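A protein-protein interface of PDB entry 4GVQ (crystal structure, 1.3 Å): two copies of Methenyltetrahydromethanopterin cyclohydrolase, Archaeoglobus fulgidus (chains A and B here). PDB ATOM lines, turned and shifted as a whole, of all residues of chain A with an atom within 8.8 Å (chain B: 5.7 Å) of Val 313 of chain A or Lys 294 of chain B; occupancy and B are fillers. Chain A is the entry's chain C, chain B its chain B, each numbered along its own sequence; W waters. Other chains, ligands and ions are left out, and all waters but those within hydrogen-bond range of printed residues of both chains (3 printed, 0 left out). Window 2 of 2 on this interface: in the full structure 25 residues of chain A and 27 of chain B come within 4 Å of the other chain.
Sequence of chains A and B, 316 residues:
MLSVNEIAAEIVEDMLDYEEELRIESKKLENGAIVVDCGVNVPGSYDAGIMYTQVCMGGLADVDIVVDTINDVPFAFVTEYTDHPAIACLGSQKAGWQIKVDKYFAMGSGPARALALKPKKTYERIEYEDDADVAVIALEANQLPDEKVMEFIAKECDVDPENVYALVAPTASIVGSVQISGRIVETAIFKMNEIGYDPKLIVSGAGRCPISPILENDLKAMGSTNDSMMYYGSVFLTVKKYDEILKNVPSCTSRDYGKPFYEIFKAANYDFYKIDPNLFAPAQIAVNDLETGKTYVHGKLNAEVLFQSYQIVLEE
ND2 of Asn 288 of chain B lies close to N of Ile 214 of chain A, 2.8 Å away.
The side-chain amide oxygen (OE1) of Gln 311 of chain A lies close to the backbone carbonyl oxygen (O) of Gly 293 of chain B, 2.9 Å away.
The backbone NH (N) of Thr 295 of chain B is in hydrogen-bond range of the backbone carbonyl oxygen (O) of Gln 311 of chain A, at 3.1 Å.
The backbone carbonyl oxygen (O) of Thr 295 of chain B lies within hydrogen-bond range of the backbone NH (N) of Val 313 of chain A (2.8 Å).
N of Val 297 of chain B lies within hydrogen-bond range of O of Val 313 of chain A (3.0 Å).
OE1 of Glu 216 of chain A lies close to O of Thr 292 of chain B (3.5 Å).
N of Val 287 of chain B is in hydrogen-bond range of O of Tyr 296 of chain B.
N of Asp 289 of chain B is in hydrogen-bond range of O of Lys 294 of chain B (2.8 Å).
The side-chain hydroxyl of Tyr 296 of chain B lies within hydrogen-bond range of the side-chain amino group of Lys 294 of chain B, 3.2 Å away.
The side-chain amino group (NZ) of Lys 220 of chain A is in salt-bridge range of the side-chain carboxylate (OE2) of Glu 216 of chain A.
The side-chain amide oxygen of Gln 311 of chain A lies close to the side-chain carboxylate of Glu 216 of chain A, at 3.0 Å.
The side-chain amino group (NZ) of Lys 220 of chain A lies close to the side-chain amide nitrogen (NE2) of Gln 311 of chain A, at 2.8 Å.
Val 73 of chain A touches Val 297 of chain B (CG1 to CG2, 3.8 Å).
OG1 of Thr 295 of chain B touches CB of Pro 213 of chain A (3.3 Å).
CB of Ile 214 of chain A touches CD2 of Leu 290 of chain B, at 3.6 Å.
Gly 293 of chain B touches Ile 214 of chain A.
Leu 215 of chain A touches Gly 293 of chain B (CD2 to O, 3.4 Å).
CA of Gly 293 of chain B touches OE1 of Glu 216 of chain A, at 3.8 Å.
CA of Lys 294 of chain B touches O of Gln 311 of chain A, at 3.6 Å.
Thr 295 of chain B touches Ile 312 of chain A.
Ile 312 of chain A touches Val 297 of chain B.
Val 297 of chain B touches Glu 315 of chain A (O to CG, 3.6 Å).
Phe 307 of chain A touches none of the printed residues of chain B.
Of the printed residues of chain B, Gln 311 of chain A touches Gly 293, Lys 294 and Thr 295.
Of chain B, only Lys 294, Thr 295, Tyr 296 and Val 297 come within 4 Å of Val 313 of chain A.
Printed residues of chain A within 4 Å of Thr 292 of chain B: Glu 216.
Of the printed residues of chain A, Gly 293 of chain B touches Ile 214 (3.9 Å), Leu 215 (3.4 Å), Glu 216 (3.8 Å) and Gln 311 (2.9 Å).
Hydrophobic or aromatic side chains of chain A within 4 Å of the printed part of chain B: Val 73, Pro 213, Ile 214, Leu 215, Ile 312, Val 313 and Leu 314.
Along chain A the printed residues that touch a printed residue of chain B span positions 73 to 315.
Of the 10 printed residues of chain B, 8 touch a printed residue of chain A.
Along chain B the printed residues that touch a printed residue of chain A span positions 288 to 297.
No position is printed for both chains.
Of the 20 pairs that touch across the chains among the printed residues, none has its exchanged pair printed and touching as well.
Water W3 lies within hydrogen-bond range of OG1 of Thr 295 of chain B (2.7 Å), O of Tyr 310 of chain A (2.7 Å) and O of Gly 293 of chain B (2.7 Å).
Water W1 bridges the backbone carbonyl oxygen of Val 313 of chain A and the backbone carbonyl oxygen of Val 297 of chain B.
Water W2 lies within hydrogen-bond range of N of Glu 315 of chain A (2.9 Å) and O of Val 297 of chain B (3.0 Å).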
ATOM      1  N   VAL A  73      -0.032   9.389  26.159  1.00  0.00           N
ATOM      2  CA  VAL A  73       1.198   9.898  26.753  1.00  0.00           C
ATOM      3  C   VAL A  73       1.570  11.175  25.998  1.00  0.00           C
ATOM      4  O   VAL A  73       1.606  11.169  24.772  1.00  0.00           O
ATOM      5  CB  VAL A  73       2.372   8.919  26.616  1.00  0.00           C
ATOM      6  CG1 VAL A  73       3.661   9.530  27.166  1.00  0.00           C
ATOM      7  CG2 VAL A  73       2.029   7.616  27.282  1.00  0.00           C
ATOM      8  N   PHE A  75       3.643  14.118  24.278  1.00  0.00           N
ATOM      9  CA  PHE A  75       4.941  14.389  23.646  1.00  0.00           C
ATOM     10  C   PHE A  75       4.850  15.715  22.931  1.00  0.00           C
ATOM     11  O   PHE A  75       3.779  16.121  22.473  1.00  0.00           O
ATOM     12  CB  PHE A  75       5.313  13.310  22.609  1.00  0.00           C
ATOM     13  CG  PHE A  75       5.567  11.968  23.232  1.00  0.00           C
ATOM     14  CD1 PHE A  75       4.557  11.007  23.304  1.00  0.00           C
ATOM     15  CD2 PHE A  75       6.796  11.683  23.842  1.00  0.00           C
ATOM     16  CE1 PHE A  75       4.798   9.783  23.902  1.00  0.00           C
ATOM     17  CE2 PHE A  75       7.056  10.442  24.415  1.00  0.00           C
ATOM     18  CZ  PHE A  75       6.053   9.501  24.462  1.00  0.00           C
ATOM     19  N   PRO A 213      12.411  12.116  23.702  1.00  0.00           N
ATOM     20  CA  PRO A 213      13.066  12.447  24.958  1.00  0.00           C
ATOM     21  C   PRO A 213      14.582  12.388  24.776  1.00  0.00           C
ATOM     22  O   PRO A 213      15.087  11.732  23.870  1.00  0.00           O
ATOM     23  CB  PRO A 213      12.607  11.331  25.907  1.00  0.00           C
ATOM     24  CG  PRO A 213      11.376  10.779  25.263  1.00  0.00           C
ATOM     25  CD  PRO A 213      11.550  10.922  23.781  1.00  0.00           C
ATOM     26  N   ILE A 214      15.296  13.085  25.640  1.00  0.00           N
ATOM     27  CA  ILE A 214      16.753  13.072  25.582  1.00  0.00           C
ATOM     28  C   ILE A 214      17.239  11.859  26.377  1.00  0.00           C
ATOM     29  O   ILE A 214      16.960  11.744  27.575  1.00  0.00           O
ATOM     30  CB  ILE A 214      17.329  14.378  26.158  1.00  0.00           C
ATOM     31  CG1 ILE A 214      16.814  15.584  25.340  1.00  0.00           C
ATOM     32  CG2 ILE A 214      18.848  14.308  26.166  1.00  0.00           C
ATOM     33  CD1 ILE A 214      17.076  16.906  25.994  1.00  0.00           C
ATOM     34  N   LEU A 215      17.938  10.946  25.700  1.00  0.00           N
ATOM     35  CA  LEU A 215      18.452   9.741  26.354  1.00  0.00           C
ATOM     36  C   LEU A 215      19.830  10.021  26.943  1.00  0.00           C
ATOM     37  O   LEU A 215      20.315  11.156  26.857  1.00  0.00           O
ATOM     38  CB  LEU A 215      18.439   8.547  25.405  1.00  0.00           C
ATOM     39  CG  LEU A 215      17.098   8.122  24.814  1.00  0.00           C
ATOM     40  CD1 LEU A 215      17.152   6.685  24.309  1.00  0.00           C
ATOM     41  CD2 LEU A 215      15.822   8.413  25.557  1.00  0.00           C
ATOM     42  N   GLU A 216      20.466   9.012  27.534  1.00  0.00           N
ATOM     43  CA  GLU A 216      21.560   9.265  28.446  1.00  0.00           C
ATOM     44  C   GLU A 216      22.924   9.465  27.798  1.00  0.00           C
ATOM     45  O   GLU A 216      23.883   9.841  28.474  1.00  0.00           O
ATOM     46  CB  GLU A 216      21.600   8.194  29.548  1.00  0.00           C
ATOM     47  CG  GLU A 216      22.017   6.813  29.069  1.00  0.00           C
ATOM     48  CD  GLU A 216      20.842   5.940  28.669  1.00  0.00           C
ATOM     49  OE1 GLU A 216      19.761   6.408  28.207  1.00  0.00           O
ATOM     50  OE2 GLU A 216      21.028   4.719  28.788  1.00  0.00           O
ATOM     51  N   LYS A 220      22.646   6.231  22.366  1.00  0.00           N
ATOM     52  CA  LYS A 220      21.220   5.957  22.609  1.00  0.00           C
ATOM     53  C   LYS A 220      20.333   6.971  21.892  1.00  0.00           C
ATOM     54  O   LYS A 220      19.299   6.641  21.299  1.00  0.00           O
ATOM     55  CB  LYS A 220      20.915   5.960  24.119  1.00  0.00           C
ATOM     56  CG  LYS A 220      21.449   4.759  24.874  1.00  0.00           C
ATOM     57  CD  LYS A 220      20.550   3.558  24.721  1.00  0.00           C
ATOM     58  CE  LYS A 220      20.790   2.472  25.781  1.00  0.00           C
ATOM     59  NZ  LYS A 220      20.186   2.760  27.111  1.00  0.00           N
ATOM     60  N   PHE A 307       7.839   3.263  22.105  1.00  0.00           N
ATOM     61  CA  PHE A 307       7.918   3.401  23.555  1.00  0.00           C
ATOM     62  C   PHE A 307       9.130   2.638  24.116  1.00  0.00           C
ATOM     63  O   PHE A 307       9.710   3.063  25.110  1.00  0.00           O
ATOM     64  CB  PHE A 307       6.635   2.932  24.213  1.00  0.00           C
ATOM     65  CG  PHE A 307       5.550   3.966  24.247  1.00  0.00           C
ATOM     66  CD1 PHE A 307       5.489   5.017  23.312  1.00  0.00           C
ATOM     67  CD2 PHE A 307       4.561   3.891  25.217  1.00  0.00           C
ATOM     68  CE1 PHE A 307       4.450   5.950  23.359  1.00  0.00           C
ATOM     69  CE2 PHE A 307       3.524   4.815  25.244  1.00  0.00           C
ATOM     70  CZ  PHE A 307       3.474   5.839  24.319  1.00  0.00           C
ATOM     71  N   GLN A 308       9.517   1.527  23.472  1.00  0.00           N
ATOM     72  CA  GLN A 308      10.768   0.844  23.827  1.00  0.00           C
ATOM     73  C   GLN A 308      11.940   1.762  23.540  1.00  0.00           C
ATOM     74  O   GLN A 308      12.805   1.945  24.419  1.00  0.00           O
ATOM     75  CB  GLN A 308      10.926  -0.474  23.030  1.00  0.00           C
ATOM     76  CG  GLN A 308       9.888  -1.564  23.284  1.00  0.00           C
ATOM     77  CD  GLN A 308       9.903  -2.610  22.184  1.00  0.00           C
ATOM     78  OE1 GLN A 308      10.886  -2.724  21.441  1.00  0.00           O
ATOM     79  NE2 GLN A 308       8.802  -3.362  22.046  1.00  0.00           N
ATOM     80  N   SER A 309      11.978   2.349  22.342  1.00  0.00           N
ATOM     81  CA  SER A 309      13.080   3.229  21.937  1.00  0.00           C
ATOM     82  C   SER A 309      13.239   4.412  22.897  1.00  0.00           C
ATOM     83  O   SER A 309      14.346   4.814  23.251  1.00  0.00           O
ATOM     84  CB  SER A 309      12.773   3.780  20.573  1.00  0.00           C
ATOM     85  OG  SER A 309      13.822   4.598  20.181  1.00  0.00           O
ATOM     86  N   TYR A 310      12.107   4.981  23.289  1.00  0.00           N
ATOM     87  CA  TYR A 310      12.050   6.165  24.120  1.00  0.00           C
ATOM     88  C   TYR A 310      12.279   5.883  25.594  1.00  0.00           C
ATOM     89  O   TYR A 310      12.247   6.804  26.412  1.00  0.00           O
ATOM     90  CB  TYR A 310      10.680   6.832  23.922  1.00  0.00           C
ATOM     91  CG  TYR A 310      10.477   7.684  22.698  1.00  0.00           C
ATOM     92  CD1 TYR A 310      11.415   7.763  21.693  1.00  0.00           C
ATOM     93  CD2 TYR A 310       9.334   8.471  22.609  1.00  0.00           C
ATOM     94  CE1 TYR A 310      11.253   8.594  20.587  1.00  0.00           C
ATOM     95  CE2 TYR A 310       9.124   9.320  21.541  1.00  0.00           C
ATOM     96  CZ  TYR A 310      10.087   9.394  20.527  1.00  0.00           C
ATOM     97  OH  TYR A 310       9.866  10.249  19.486  1.00  0.00           O
ATOM     98  N   GLN A 311      12.474   4.618  25.959  1.00  0.00           N
ATOM     99  CA  GLN A 311      12.722   4.275  27.347  1.00  0.00           C
ATOM    100  C   GLN A 311      11.621   4.798  28.263  1.00  0.00           C
ATOM    101  O   GLN A 311      11.870   5.318  29.355  1.00  0.00           O
ATOM    102  CB  GLN A 311      14.138   4.724  27.772  1.00  0.00           C
ATOM    103  CG  GLN A 311      15.204   4.097  26.855  1.00  0.00           C
ATOM    104  CD  GLN A 311      16.640   4.337  27.246  1.00  0.00           C
ATOM    105  OE1 GLN A 311      16.997   5.342  27.906  1.00  0.00           O
ATOM    106  NE2 GLN A 311      17.488   3.446  26.794  1.00  0.00           N
ATOM    107  N   ILE A 312      10.385   4.602  27.816  1.00  0.00           N
ATOM    108  CA  ILE A 312       9.193   4.966  28.576  1.00  0.00           C
ATOM    109  C   ILE A 312       8.987   3.994  29.726  1.00  0.00           C
ATOM    110  O   ILE A 312       9.054   2.766  29.541  1.00  0.00           O
ATOM    111  CB  ILE A 312       7.944   4.916  27.684  1.00  0.00           C
ATOM    112  CG1 ILE A 312       8.051   5.946  26.560  1.00  0.00           C
ATOM    113  CG2 ILE A 312       6.660   5.042  28.512  1.00  0.00           C
ATOM    114  CD1 ILE A 312       8.128   7.381  27.011  1.00  0.00           C
ATOM    115  N   VAL A 313       8.683   4.526  30.899  1.00  0.00           N
ATOM    116  CA  VAL A 313       8.301   3.728  32.057  1.00  0.00           C
ATOM    117  C   VAL A 313       6.876   4.064  32.430  1.00  0.00           C
ATOM    118  O   VAL A 313       6.592   5.185  32.874  1.00  0.00           O
ATOM    119  CB  VAL A 313       9.224   4.022  33.267  1.00  0.00           C
ATOM    120  CG1 VAL A 313       8.856   3.216  34.510  1.00  0.00           C
ATOM    121  CG2 VAL A 313      10.699   3.841  32.888  1.00  0.00           C
ATOM    122  N   LEU A 314       5.971   3.112  32.218  1.00  0.00           N
ATOM    123  CA  LEU A 314       4.577   3.272  32.647  1.00  0.00           C
ATOM    124  C   LEU A 314       4.436   2.671  34.050  1.00  0.00           C
ATOM    125  O   LEU A 314       5.212   1.802  34.457  1.00  0.00           O
ATOM    126  CB  LEU A 314       3.632   2.552  31.681  1.00  0.00           C
ATOM    127  CG  LEU A 314       3.743   2.880  30.188  1.00  0.00           C
ATOM    128  CD1 LEU A 314       2.785   2.005  29.386  1.00  0.00           C
ATOM    129  CD2 LEU A 314       3.438   4.348  29.947  1.00  0.00           C
ATOM    130  N   GLU A 315       3.422   3.109  34.784  1.00  0.00           N
ATOM    131  CA  GLU A 315       3.175   2.586  36.136  1.00  0.00           C
ATOM    132  C   GLU A 315       2.699   1.132  36.109  1.00  0.00           C
ATOM    133  O   GLU A 315       2.062   0.697  35.143  1.00  0.00           O
ATOM    134  CB  GLU A 315       2.142   3.451  36.857  1.00  0.00           C
ATOM    135  CG  GLU A 315       2.614   4.880  37.095  1.00  0.00           C
ATOM    136  CD  GLU A 315       1.569   5.754  37.742  1.00  0.00           C
ATOM    137  OE1 GLU A 315       0.400   5.326  37.878  1.00  0.00           O
ATOM    138  OE2 GLU A 315       1.923   6.879  38.112  1.00  0.00           O
ATOM    139  N   VAL B 287       7.768  12.596  32.332  1.00  0.00           N
ATOM    140  CA  VAL B 287       8.944  13.273  32.908  1.00  0.00           C
ATOM    141  C   VAL B 287      10.219  12.607  32.376  1.00  0.00           C
ATOM    142  O   VAL B 287      10.532  11.459  32.744  1.00  0.00           O
ATOM    143  CB  VAL B 287       8.944  13.204  34.442  1.00  0.00           C
ATOM    144  CG1 VAL B 287      10.163  13.938  35.017  1.00  0.00           C
ATOM    145  CG2 VAL B 287       7.643  13.756  35.030  1.00  0.00           C
ATOM    146  N   ASN B 288      10.915  13.290  31.465  1.00  0.00           N
ATOM    147  CA  ASN B 288      12.161  12.814  30.892  1.00  0.00           C
ATOM    148  C   ASN B 288      13.288  13.184  31.855  1.00  0.00           C
ATOM    149  O   ASN B 288      13.575  14.360  32.083  1.00  0.00           O
ATOM    150  CB  ASN B 288      12.341  13.460  29.529  1.00  0.00           C
ATOM    151  CG  ASN B 288      13.695  13.183  28.883  1.00  0.00           C
ATOM    152  OD1 ASN B 288      14.375  12.160  29.148  1.00  0.00           O
ATOM    153  ND2 ASN B 288      14.057  14.042  27.971  1.00  0.00           N
ATOM    154  N   ASP B 289      13.915  12.159  32.419  1.00  0.00           N
ATOM    155  CA  ASP B 289      15.004  12.318  33.371  1.00  0.00           C
ATOM    156  C   ASP B 289      16.335  12.311  32.625  1.00  0.00           C
ATOM    157  O   ASP B 289      16.735  11.282  32.066  1.00  0.00           O
ATOM    158  CB  ASP B 289      14.983  11.129  34.354  1.00  0.00           C
ATOM    159  CG  ASP B 289      16.193  11.098  35.279  1.00  0.00           C
ATOM    160  OD1 ASP B 289      16.750  12.189  35.540  1.00  0.00           O
ATOM    161  OD2 ASP B 289      16.558  10.003  35.778  1.00  0.00           O
ATOM    162  N   LEU B 290      17.018  13.448  32.618  1.00  0.00           N
ATOM    163  CA  LEU B 290      18.295  13.520  31.906  1.00  0.00           C
ATOM    164  C   LEU B 290      19.360  12.584  32.499  1.00  0.00           C
ATOM    165  O   LEU B 290      20.238  12.112  31.776  1.00  0.00           O
ATOM    166  CB  LEU B 290      18.811  14.957  31.876  1.00  0.00           C
ATOM    167  CG  LEU B 290      17.946  15.910  31.056  1.00  0.00           C
ATOM    168  CD1 LEU B 290      18.552  17.305  31.134  1.00  0.00           C
ATOM    169  CD2 LEU B 290      17.779  15.419  29.618  1.00  0.00           C
ATOM    170  N   THR B 292      19.170   9.492  33.840  1.00  0.00           N
ATOM    171  CA  THR B 292      19.075   8.085  33.453  1.00  0.00           C
ATOM    172  C   THR B 292      18.618   7.895  32.023  1.00  0.00           C
ATOM    173  O   THR B 292      18.726   6.790  31.492  1.00  0.00           O
ATOM    174  CB  THR B 292      18.058   7.316  34.322  1.00  0.00           C
ATOM    175  OG1 THR B 292      16.738   7.913  34.195  1.00  0.00           O
ATOM    176  CG2 THR B 292      18.484   7.289  35.763  1.00  0.00           C
ATOM    177  N   GLY B 293      18.100   8.941  31.397  1.00  0.00           N
ATOM    178  CA  GLY B 293      17.536   8.833  30.056  1.00  0.00           C
ATOM    179  C   GLY B 293      16.179   8.143  29.978  1.00  0.00           C
ATOM    180  O   GLY B 293      15.744   7.789  28.886  1.00  0.00           O
ATOM    181  N   LYS B 294      15.536   7.927  31.133  1.00  0.00           N
ATOM    182  CA  LYS B 294      14.192   7.308  31.158  1.00  0.00           C
ATOM    183  C   LYS B 294      13.123   8.395  31.154  1.00  0.00           C
ATOM    184  O   LYS B 294      13.394   9.539  31.523  1.00  0.00           O
ATOM    185  CB  LYS B 294      14.052   6.429  32.396  1.00  0.00           C
ATOM    186  CG  LYS B 294      15.029   5.261  32.359  1.00  0.00           C
ATOM    187  CD  LYS B 294      15.285   4.619  33.707  1.00  0.00           C
ATOM    188  CE  LYS B 294      14.071   3.890  34.205  1.00  0.00           C
ATOM    189  NZ  LYS B 294      14.385   3.237  35.508  1.00  0.00           N
ATOM    190  N   THR B 295      11.915   8.043  30.727  1.00  0.00           N
ATOM    191  CA  THR B 295      10.792   8.977  30.755  1.00  0.00           C
ATOM    192  C   THR B 295       9.644   8.304  31.491  1.00  0.00           C
ATOM    193  O   THR B 295       9.111   7.287  31.040  1.00  0.00           O
ATOM    194  CB  THR B 295      10.369   9.465  29.368  1.00  0.00           C
ATOM    195  OG1 THR B 295      11.421  10.286  28.831  1.00  0.00           O
ATOM    196  CG2 THR B 295       9.089  10.304  29.442  1.00  0.00           C
ATOM    197  N   TYR B 296       9.257   8.898  32.621  1.00  0.00           N
ATOM    198  CA  TYR B 296       8.251   8.302  33.513  1.00  0.00           C
ATOM    199  C   TYR B 296       6.907   8.914  33.281  1.00  0.00           C
ATOM    200  O   TYR B 296       6.804  10.158  33.295  1.00  0.00           O
ATOM    201  CB  TYR B 296       8.646   8.507  34.969  1.00  0.00           C
ATOM    202  CG  TYR B 296       9.942   7.850  35.385  1.00  0.00           C
ATOM    203  CD1 TYR B 296      11.191   8.493  35.212  1.00  0.00           C
ATOM    204  CD2 TYR B 296       9.915   6.626  36.035  1.00  0.00           C
ATOM    205  CE1 TYR B 296      12.377   7.899  35.636  1.00  0.00           C
ATOM    206  CE2 TYR B 296      11.094   6.016  36.438  1.00  0.00           C
ATOM    207  CZ  TYR B 296      12.309   6.658  36.247  1.00  0.00           C
ATOM    208  OH  TYR B 296      13.465   6.061  36.707  1.00  0.00           O
ATOM    209  N   VAL B 297       5.887   8.088  33.088  1.00  0.00           N
ATOM    210  CA  VAL B 297       4.541   8.594  32.788  1.00  0.00           C
ATOM    211  C   VAL B 297       3.641   8.378  33.989  1.00  0.00           C
ATOM    212  O   VAL B 297       3.604   7.285  34.583  1.00  0.00           O
ATOM    213  CB  VAL B 297       3.968   7.875  31.552  1.00  0.00           C
ATOM    214  CG1 VAL B 297       2.589   8.412  31.212  1.00  0.00           C
ATOM    215  CG2 VAL B 297       4.935   8.000  30.372  1.00  0.00           C
HETATM  216  O   HOH W   1       5.859   5.812  35.517  1.00  0.00           O
HETATM  217  O   HOH W   2       1.786   5.165  33.568  1.00  0.00           O
HETATM  218  O   HOH W   3      13.440   8.824  27.805  1.00  0.00           O
